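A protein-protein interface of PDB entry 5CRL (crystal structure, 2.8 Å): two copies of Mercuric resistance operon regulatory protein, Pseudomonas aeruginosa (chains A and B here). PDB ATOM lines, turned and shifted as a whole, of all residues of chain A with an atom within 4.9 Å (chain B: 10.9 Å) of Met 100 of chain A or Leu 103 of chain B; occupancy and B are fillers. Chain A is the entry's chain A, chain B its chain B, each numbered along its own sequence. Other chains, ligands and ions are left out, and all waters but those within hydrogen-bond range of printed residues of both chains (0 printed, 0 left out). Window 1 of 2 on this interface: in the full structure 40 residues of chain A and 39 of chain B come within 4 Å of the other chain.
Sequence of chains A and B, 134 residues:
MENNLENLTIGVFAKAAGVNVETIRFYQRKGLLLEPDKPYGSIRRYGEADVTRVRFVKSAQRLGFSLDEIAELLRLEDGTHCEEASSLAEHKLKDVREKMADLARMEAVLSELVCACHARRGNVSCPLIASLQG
Of the 18 printed residues of chain B, 6 touch a printed residue of chain A.
Hydrophobic or aromatic side chains of chain A that line the printed part of chain B: Val 96, Met 100, Leu 103 and Ala 104.
Of the printed residues of chain B, Met 100 of chain A touches Leu 103.
Leu 103 of chain B touches just these residues of chain A: Val 96 (3.4 Å), Lys 99 (3.9 Å), Met 100 (3.7 Å) and Leu 103 (3.2 Å).
Of chain B, only Leu 103 (3.9 Å) comes within 4 Å of Lys 99 of chain A.
No residue of chain B comes within 4 Å of Ala 101 of chain A.
No residue of chain B comes within 4 Å of Asp 102 of chain A.
Printed residues of chain B within 4 Å of Leu 103 of chain A: Val 96 (3.4 Å), Lys 99 (3.9 Å), Met 100 (3.5 Å) and Leu 103 (3.2 Å).
Of the printed residues of chain A, Ser 111 of chain B touches Arg 97 (3.1 Å).
Of the printed residues of chain A, Met 100 of chain B touches Leu 103 (3.5 Å) and Ala 104 (3.9 Å).
Met 106 of chain B touches none of the printed residues of chain A.
Val 109 of chain B touches none of the printed residues of chain A.
The nearest printed residue of chain B that does not touch Met 100 of chain A is Ala 104 of chain B (4.001 Å).
The nearest printed residue of chain A that does not touch Leu 103 of chain B is Arg 97 of chain A (6.3 Å).
The nearest printed residue of chain A that does not touch Met 100 of chain B is Met 100 of chain A (4.1 Å).
The side-chain carboxylate (OE2) of Glu 107 of chain B is in salt-bridge range of the guanidinium group (NH2) of Arg 97 of chain A, 2.7 Å away.
OG of Ser 111 of chain B sits at hydrogen-bond distance from NH2 of Arg 97 of chain A (3.1 Å).
Val 96 of chain A touches Leu 103 of chain B, and with the chains exchanged Leu 103 of chain A touches Val 96 of chain B.
Lys 99 of chain A touches Leu 103 of chain B, and with the chains exchanged Leu 103 of chain A touches Lys 99 of chain B.
Met 100 of chain A touches Leu 103 of chain B, and with the chains exchanged Leu 103 of chain A touches Met 100 of chain B.
Leu 103 of chain A touches its own counterpart, Leu 103 of chain B.
Positions printed for both chains: 96, 97, 98, 99, 100, 101, 102, 103 and 104.
Of the 11 pairs that touch across the chains among the printed residues, 7 have their exchanged pair printed and touching as well.
The backbone carbonyl oxygen (O) of Glu 107 of chain B sits at hydrogen-bond distance from the side-chain hydroxyl (OG) of Ser 111 of chain B (2.7 Å).
Among the printed residues, merely in contact across the chains: Leu 103 of chain A with Leu 103 of chain B, Leu 103 of chain A with Val 96 of chain B, Val 96 of chain A with Leu 103 of chain B, Leu 103 of chain A with Met 100 of chain B, Met 100 of chain A with Leu 103 of chain B, Lys 99 of chain A with Leu 103 of chain B, Leu 103 of chain A with Lys 99 of chain B, Val 96 of chain A with Glu 107 of chain B and Ala 104 of chain A with Met 100 of chain B.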
ATOM      1  N   VAL A  96      10.058  12.239 -18.657  1.00  0.00           N
ATOM      2  CA  VAL A  96       9.531  12.902 -19.825  1.00  0.00           C
ATOM      3  C   VAL A  96       8.861  11.874 -20.738  1.00  0.00           C
ATOM      4  O   VAL A  96       7.733  12.075 -21.189  1.00  0.00           O
ATOM      5  CB  VAL A  96      10.633  13.670 -20.585  1.00  0.00           C
ATOM      6  CG1 VAL A  96      10.111  14.199 -21.914  1.00  0.00           C
ATOM      7  CG2 VAL A  96      11.164  14.834 -19.752  1.00  0.00           C
ATOM      8  N   ARG A  97       9.553  10.765 -20.992  1.00  0.00           N
ATOM      9  CA  ARG A  97       9.049   9.722 -21.908  1.00  0.00           C
ATOM     10  C   ARG A  97       7.771   9.047 -21.437  1.00  0.00           C
ATOM     11  O   ARG A  97       6.892   8.758 -22.250  1.00  0.00           O
ATOM     12  CB  ARG A  97      10.125   8.678 -22.171  1.00  0.00           C
ATOM     13  CG  ARG A  97      11.183   9.205 -23.100  1.00  0.00           C
ATOM     14  CD  ARG A  97      12.421   8.350 -23.145  1.00  0.00           C
ATOM     15  NE  ARG A  97      13.249   8.816 -24.255  1.00  0.00           N
ATOM     16  CZ  ARG A  97      14.545   8.556 -24.409  1.00  0.00           C
ATOM     17  NH1 ARG A  97      15.204   7.801 -23.528  1.00  0.00           N
ATOM     18  NH2 ARG A  97      15.180   9.061 -25.462  1.00  0.00           N
ATOM     19  N   GLU A  98       7.670   8.807 -20.134  1.00  0.00           N
ATOM     20  CA  GLU A  98       6.440   8.299 -19.552  1.00  0.00           C
ATOM     21  C   GLU A  98       5.313   9.275 -19.842  1.00  0.00           C
ATOM     22  O   GLU A  98       4.279   8.901 -20.406  1.00  0.00           O
ATOM     23  CB  GLU A  98       6.588   8.123 -18.046  1.00  0.00           C
ATOM     24  CG  GLU A  98       7.476   6.953 -17.637  1.00  0.00           C
ATOM     25  CD  GLU A  98       7.600   6.794 -16.121  1.00  0.00           C
ATOM     26  OE1 GLU A  98       6.586   7.003 -15.412  1.00  0.00           O
ATOM     27  OE2 GLU A  98       8.708   6.458 -15.637  1.00  0.00           O
ATOM     28  N   LYS A  99       5.533  10.537 -19.473  1.00  0.00           N
ATOM     29  CA  LYS A  99       4.532  11.576 -19.692  1.00  0.00           C
ATOM     30  C   LYS A  99       4.103  11.656 -21.150  1.00  0.00           C
ATOM     31  O   LYS A  99       2.909  11.759 -21.437  1.00  0.00           O
ATOM     32  CB  LYS A  99       5.030  12.927 -19.198  1.00  0.00           C
ATOM     33  CG  LYS A  99       4.687  13.187 -17.746  1.00  0.00           C
ATOM     34  CD  LYS A  99       5.729  14.065 -17.070  1.00  0.00           C
ATOM     35  CE  LYS A  99       5.283  14.515 -15.682  1.00  0.00           C
ATOM     36  NZ  LYS A  99       6.391  15.167 -14.927  1.00  0.00           N
ATOM     37  N   MET A 100       5.059  11.577 -22.068  1.00  0.00           N
ATOM     38  CA  MET A 100       4.738  11.572 -23.500  1.00  0.00           C
ATOM     39  C   MET A 100       3.911  10.356 -23.900  1.00  0.00           C
ATOM     40  O   MET A 100       3.010  10.459 -24.726  1.00  0.00           O
ATOM     41  CB  MET A 100       6.009  11.569 -24.339  1.00  0.00           C
ATOM     42  CG  MET A 100       6.832  12.835 -24.225  1.00  0.00           C
ATOM     43  SD  MET A 100       8.267  12.796 -25.305  1.00  0.00           S
ATOM     44  CE  MET A 100       7.440  12.875 -26.895  1.00  0.00           C
ATOM     45  N   ALA A 101       4.239   9.200 -23.322  1.00  0.00           N
ATOM     46  CA  ALA A 101       3.507   7.974 -23.599  1.00  0.00           C
ATOM     47  C   ALA A 101       2.075   8.075 -23.079  1.00  0.00           C
ATOM     48  O   ALA A 101       1.141   7.622 -23.734  1.00  0.00           O
ATOM     49  CB  ALA A 101       4.222   6.789 -22.993  1.00  0.00           C
ATOM     50  N   ASP A 102       1.888   8.700 -21.921  1.00  0.00           N
ATOM     51  CA  ASP A 102       0.538   8.939 -21.431  1.00  0.00           C
ATOM     52  C   ASP A 102      -0.206   9.909 -22.345  1.00  0.00           C
ATOM     53  O   ASP A 102      -1.274   9.579 -22.846  1.00  0.00           O
ATOM     54  CB  ASP A 102       0.538   9.432 -19.983  1.00  0.00           C
ATOM     55  CG  ASP A 102       0.994   8.353 -19.001  1.00  0.00           C
ATOM     56  OD1 ASP A 102       0.693   7.149 -19.226  1.00  0.00           O
ATOM     57  OD2 ASP A 102       1.654   8.710 -17.999  1.00  0.00           O
ATOM     58  N   LEU A 103       0.344  11.100 -22.564  1.00  0.00           N
ATOM     59  CA  LEU A 103      -0.304  12.083 -23.450  1.00  0.00           C
ATOM     60  C   LEU A 103      -0.639  11.495 -24.825  1.00  0.00           C
ATOM     61  O   LEU A 103      -1.656  11.841 -25.427  1.00  0.00           O
ATOM     62  CB  LEU A 103       0.579  13.314 -23.620  1.00  0.00           C
ATOM     63  CG  LEU A 103       0.711  14.237 -22.399  1.00  0.00           C
ATOM     64  CD1 LEU A 103       1.904  15.165 -22.569  1.00  0.00           C
ATOM     65  CD2 LEU A 103      -0.546  15.063 -22.170  1.00  0.00           C
ATOM     66  N   ALA A 104       0.221  10.601 -25.313  1.00  0.00           N
ATOM     67  CA  ALA A 104       0.014   9.956 -26.606  1.00  0.00           C
ATOM     68  C   ALA A 104      -1.225   9.096 -26.570  1.00  0.00           C
ATOM     69  O   ALA A 104      -1.991   9.042 -27.535  1.00  0.00           O
ATOM     70  CB  ALA A 104       1.227   9.118 -26.983  1.00  0.00           C
ATOM     71  N   ASP B  95      -4.581  21.066 -26.611  1.00  0.00           N
ATOM     72  CA  ASP B  95      -3.748  21.222 -25.412  1.00  0.00           C
ATOM     73  C   ASP B  95      -2.820  20.024 -25.179  1.00  0.00           C
ATOM     74  O   ASP B  95      -1.657  20.183 -24.792  1.00  0.00           O
ATOM     75  CB  ASP B  95      -4.625  21.465 -24.174  1.00  0.00           C
ATOM     76  CG  ASP B  95      -5.381  22.811 -24.232  1.00  0.00           C
ATOM     77  OD1 ASP B  95      -5.091  23.665 -25.108  1.00  0.00           O
ATOM     78  OD2 ASP B  95      -6.280  23.023 -23.390  1.00  0.00           O
ATOM     79  N   VAL B  96      -3.332  18.826 -25.436  1.00  0.00           N
ATOM     80  CA  VAL B  96      -2.525  17.615 -25.327  1.00  0.00           C
ATOM     81  C   VAL B  96      -1.340  17.708 -26.276  1.00  0.00           C
ATOM     82  O   VAL B  96      -0.198  17.475 -25.878  1.00  0.00           O
ATOM     83  CB  VAL B  96      -3.355  16.343 -25.622  1.00  0.00           C
ATOM     84  CG1 VAL B  96      -2.459  15.110 -25.696  1.00  0.00           C
ATOM     85  CG2 VAL B  96      -4.412  16.146 -24.544  1.00  0.00           C
ATOM     86  N   ARG B  97      -1.617  18.086 -27.517  1.00  0.00           N
ATOM     87  CA  ARG B  97      -0.579  18.159 -28.540  1.00  0.00           C
ATOM     88  C   ARG B  97       0.503  19.199 -28.250  1.00  0.00           C
ATOM     89  O   ARG B  97       1.684  18.956 -28.514  1.00  0.00           O
ATOM     90  CB  ARG B  97      -1.212  18.421 -29.900  1.00  0.00           C
ATOM     91  CG  ARG B  97      -1.905  17.196 -30.448  1.00  0.00           C
ATOM     92  CD  ARG B  97      -2.793  17.511 -31.631  1.00  0.00           C
ATOM     93  NE  ARG B  97      -3.154  16.294 -32.331  1.00  0.00           N
ATOM     94  CZ  ARG B  97      -4.152  16.176 -33.198  1.00  0.00           C
ATOM     95  NH1 ARG B  97      -4.947  17.208 -33.482  1.00  0.00           N
ATOM     96  NH2 ARG B  97      -4.368  14.989 -33.763  1.00  0.00           N
ATOM     97  N   GLU B  98       0.092  20.351 -27.723  1.00  0.00           N
ATOM     98  CA  GLU B  98       1.037  21.362 -27.288  1.00  0.00           C
ATOM     99  C   GLU B  98       1.958  20.768 -26.236  1.00  0.00           C
ATOM    100  O   GLU B  98       3.186  20.807 -26.372  1.00  0.00           O
ATOM    101  CB  GLU B  98       0.312  22.575 -26.714  1.00  0.00           C
ATOM    102  CG  GLU B  98      -0.382  23.435 -27.762  1.00  0.00           C
ATOM    103  CD  GLU B  98      -1.089  24.641 -27.157  1.00  0.00           C
ATOM    104  OE1 GLU B  98      -0.545  25.235 -26.198  1.00  0.00           O
ATOM    105  OE2 GLU B  98      -2.187  25.003 -27.651  1.00  0.00           O
ATOM    106  N   LYS B  99       1.358  20.210 -25.190  1.00  0.00           N
ATOM    107  CA  LYS B  99       2.132  19.598 -24.125  1.00  0.00           C
ATOM    108  C   LYS B  99       3.123  18.561 -24.659  1.00  0.00           C
ATOM    109  O   LYS B  99       4.279  18.525 -24.218  1.00  0.00           O
ATOM    110  CB  LYS B  99       1.208  18.968 -23.078  1.00  0.00           C
ATOM    111  CG  LYS B  99       0.813  19.916 -21.951  1.00  0.00           C
ATOM    112  CD  LYS B  99      -0.567  19.579 -21.394  1.00  0.00           C
ATOM    113  CE  LYS B  99      -0.882  20.331 -20.105  1.00  0.00           C
ATOM    114  NZ  LYS B  99      -2.312  20.167 -19.710  1.00  0.00           N
ATOM    115  N   MET B 100       2.675  17.723 -25.598  1.00  0.00           N
ATOM    116  CA  MET B 100       3.550  16.716 -26.187  1.00  0.00           C
ATOM    117  C   MET B 100       4.684  17.361 -26.959  1.00  0.00           C
ATOM    118  O   MET B 100       5.808  16.870 -26.941  1.00  0.00           O
ATOM    119  CB  MET B 100       2.785  15.809 -27.137  1.00  0.00           C
ATOM    120  CG  MET B 100       1.761  14.918 -26.473  1.00  0.00           C
ATOM    121  SD  MET B 100       0.980  13.849 -27.688  1.00  0.00           S
ATOM    122  CE  MET B 100       2.367  12.762 -28.041  1.00  0.00           C
ATOM    123  N   ALA B 101       4.377  18.451 -27.653  1.00  0.00           N
ATOM    124  CA  ALA B 101       5.380  19.177 -28.401  1.00  0.00           C
ATOM    125  C   ALA B 101       6.412  19.795 -27.458  1.00  0.00           C
ATOM    126  O   ALA B 101       7.601  19.799 -27.767  1.00  0.00           O
ATOM    127  CB  ALA B 101       4.732  20.235 -29.271  1.00  0.00           C
ATOM    128  N   ASP B 102       5.976  20.300 -26.310  1.00  0.00           N
ATOM    129  CA  ASP B 102       6.926  20.804 -25.317  1.00  0.00           C
ATOM    130  C   ASP B 102       7.780  19.700 -24.751  1.00  0.00           C
ATOM    131  O   ASP B 102       8.999  19.760 -24.849  1.00  0.00           O
ATOM    132  CB  ASP B 102       6.226  21.574 -24.193  1.00  0.00           C
ATOM    133  CG  ASP B 102       5.640  22.904 -24.674  1.00  0.00           C
ATOM    134  OD1 ASP B 102       6.249  23.560 -25.558  1.00  0.00           O
ATOM    135  OD2 ASP B 102       4.550  23.280 -24.187  1.00  0.00           O
ATOM    136  N   LEU B 103       7.150  18.668 -24.203  1.00  0.00           N
ATOM    137  CA  LEU B 103       7.904  17.497 -23.718  1.00  0.00           C
ATOM    138  C   LEU B 103       8.880  16.925 -24.762  1.00  0.00           C
ATOM    139  O   LEU B 103       9.979  16.495 -24.415  1.00  0.00           O
ATOM    140  CB  LEU B 103       6.956  16.391 -23.264  1.00  0.00           C
ATOM    141  CG  LEU B 103       6.164  16.680 -21.979  1.00  0.00           C
ATOM    142  CD1 LEU B 103       4.986  15.729 -21.857  1.00  0.00           C
ATOM    143  CD2 LEU B 103       7.025  16.581 -20.729  1.00  0.00           C
ATOM    144  N   ALA B 104       8.479  16.930 -26.031  1.00  0.00           N
ATOM    145  CA  ALA B 104       9.324  16.423 -27.110  1.00  0.00           C
ATOM    146  C   ALA B 104      10.582  17.269 -27.238  1.00  0.00           C
ATOM    147  O   ALA B 104      11.665  16.757 -27.497  1.00  0.00           O
ATOM    148  CB  ALA B 104       8.570  16.397 -28.421  1.00  0.00           C
ATOM    149  N   ARG B 105      10.433  18.568 -27.027  1.00  0.00           N
ATOM    150  CA  ARG B 105      11.553  19.521 -27.093  1.00  0.00           C
ATOM    151  C   ARG B 105      12.559  19.196 -25.999  1.00  0.00           C
ATOM    152  O   ARG B 105      13.772  19.158 -26.240  1.00  0.00           O
ATOM    153  CB  ARG B 105      11.001  20.947 -26.873  1.00  0.00           C
ATOM    154  CG  ARG B 105      11.819  22.128 -27.420  1.00  0.00           C
ATOM    155  CD  ARG B 105      12.482  22.986 -26.319  1.00  0.00           C
ATOM    156  NE  ARG B 105      11.487  23.524 -25.383  1.00  0.00           N
ATOM    157  CZ  ARG B 105      11.394  23.254 -24.073  1.00  0.00           C
ATOM    158  NH1 ARG B 105      12.273  22.474 -23.453  1.00  0.00           N
ATOM    159  NH2 ARG B 105      10.409  23.798 -23.363  1.00  0.00           N
ATOM    160  N   MET B 106      12.040  18.951 -24.802  1.00  0.00           N
ATOM    161  CA  MET B 106      12.875  18.543 -23.687  1.00  0.00           C
ATOM    162  C   MET B 106      13.574  17.218 -23.978  1.00  0.00           C
ATOM    163  O   MET B 106      14.770  17.079 -23.719  1.00  0.00           O
ATOM    164  CB  MET B 106      12.034  18.380 -22.430  1.00  0.00           C
ATOM    165  CG  MET B 106      11.444  19.657 -21.898  1.00  0.00           C
ATOM    166  SD  MET B 106      10.380  19.312 -20.487  1.00  0.00           S
ATOM    167  CE  MET B 106       9.795  20.983 -20.154  1.00  0.00           C
ATOM    168  N   GLU B 107      12.808  16.242 -24.475  1.00  0.00           N
ATOM    169  CA  GLU B 107      13.323  14.905 -24.706  1.00  0.00           C
ATOM    170  C   GLU B 107      14.466  14.909 -25.694  1.00  0.00           C
ATOM    171  O   GLU B 107      15.456  14.196 -25.505  1.00  0.00           O
ATOM    172  CB  GLU B 107      12.242  13.958 -25.210  1.00  0.00           C
ATOM    173  CG  GLU B 107      12.743  12.502 -25.179  1.00  0.00           C
ATOM    174  CD  GLU B 107      13.090  11.928 -26.527  1.00  0.00           C
ATOM    175  OE1 GLU B 107      13.178  12.697 -27.504  1.00  0.00           O
ATOM    176  OE2 GLU B 107      13.288  10.694 -26.601  1.00  0.00           O
ATOM    177  N   ALA B 108      14.340  15.729 -26.731  1.00  0.00           N
ATOM    178  CA  ALA B 108      15.363  15.805 -27.763  1.00  0.00           C
ATOM    179  C   ALA B 108      16.694  16.300 -27.212  1.00  0.00           C
ATOM    180  O   ALA B 108      17.729  15.675 -27.437  1.00  0.00           O
ATOM    181  CB  ALA B 108      14.899  16.711 -28.879  1.00  0.00           C
ATOM    182  N   VAL B 109      16.652  17.407 -26.467  1.00  0.00           N
ATOM    183  CA  VAL B 109      17.869  18.035 -25.921  1.00  0.00           C
ATOM    184  C   VAL B 109      18.478  17.205 -24.790  1.00  0.00           C
ATOM    185  O   VAL B 109      19.684  16.972 -24.754  1.00  0.00           O
ATOM    186  CB  VAL B 109      17.569  19.442 -25.388  1.00  0.00           C
ATOM    187  CG1 VAL B 109      18.837  20.092 -24.857  1.00  0.00           C
ATOM    188  CG2 VAL B 109      16.949  20.303 -26.482  1.00  0.00           C
ATOM    189  N   LEU B 110      17.633  16.740 -23.876  1.00  0.00           N
ATOM    190  CA  LEU B 110      18.071  15.836 -22.827  1.00  0.00           C
ATOM    191  C   LEU B 110      18.742  14.588 -23.420  1.00  0.00           C
ATOM    192  O   LEU B 110      19.828  14.219 -22.976  1.00  0.00           O
ATOM    193  CB  LEU B 110      16.904  15.446 -21.914  1.00  0.00           C
ATOM    194  CG  LEU B 110      16.357  16.497 -20.935  1.00  0.00           C
ATOM    195  CD1 LEU B 110      15.039  16.042 -20.318  1.00  0.00           C
ATOM    196  CD2 LEU B 110      17.354  16.822 -19.828  1.00  0.00           C
ATOM    197  N   SER B 111      18.118  13.941 -24.412  1.00  0.00           N
ATOM    198  CA  SER B 111      18.735  12.764 -25.066  1.00  0.00           C
ATOM    199  C   SER B 111      20.115  13.112 -25.582  1.00  0.00           C
ATOM    200  O   SER B 111      21.067  12.354 -25.426  1.00  0.00           O
ATOM    201  CB  SER B 111      17.907  12.266 -26.251  1.00  0.00           C
ATOM    202  OG  SER B 111      16.640  11.773 -25.843  1.00  0.00           O
ATOM    203  N   GLU B 112      20.208  14.286 -26.188  1.00  0.00           N
ATOM    204  CA  GLU B 112      21.438  14.759 -26.782  1.00  0.00           C
ATOM    205  C   GLU B 112      22.507  14.965 -25.717  1.00  0.00           C
ATOM    206  O   GLU B 112      23.675  14.624 -25.921  1.00  0.00           O
ATOM    207  CB  GLU B 112      21.151  16.071 -27.506  1.00  0.00           C
ATOM    208  CG  GLU B 112      22.247  16.560 -28.413  1.00  0.00           C
ATOM    209  CD  GLU B 112      22.575  15.595 -29.525  1.00  0.00           C
ATOM    210  OE1 GLU B 112      23.760  15.209 -29.586  1.00  0.00           O
ATOM    211  OE2 GLU B 112      21.670  15.227 -30.324  1.00  0.00           O
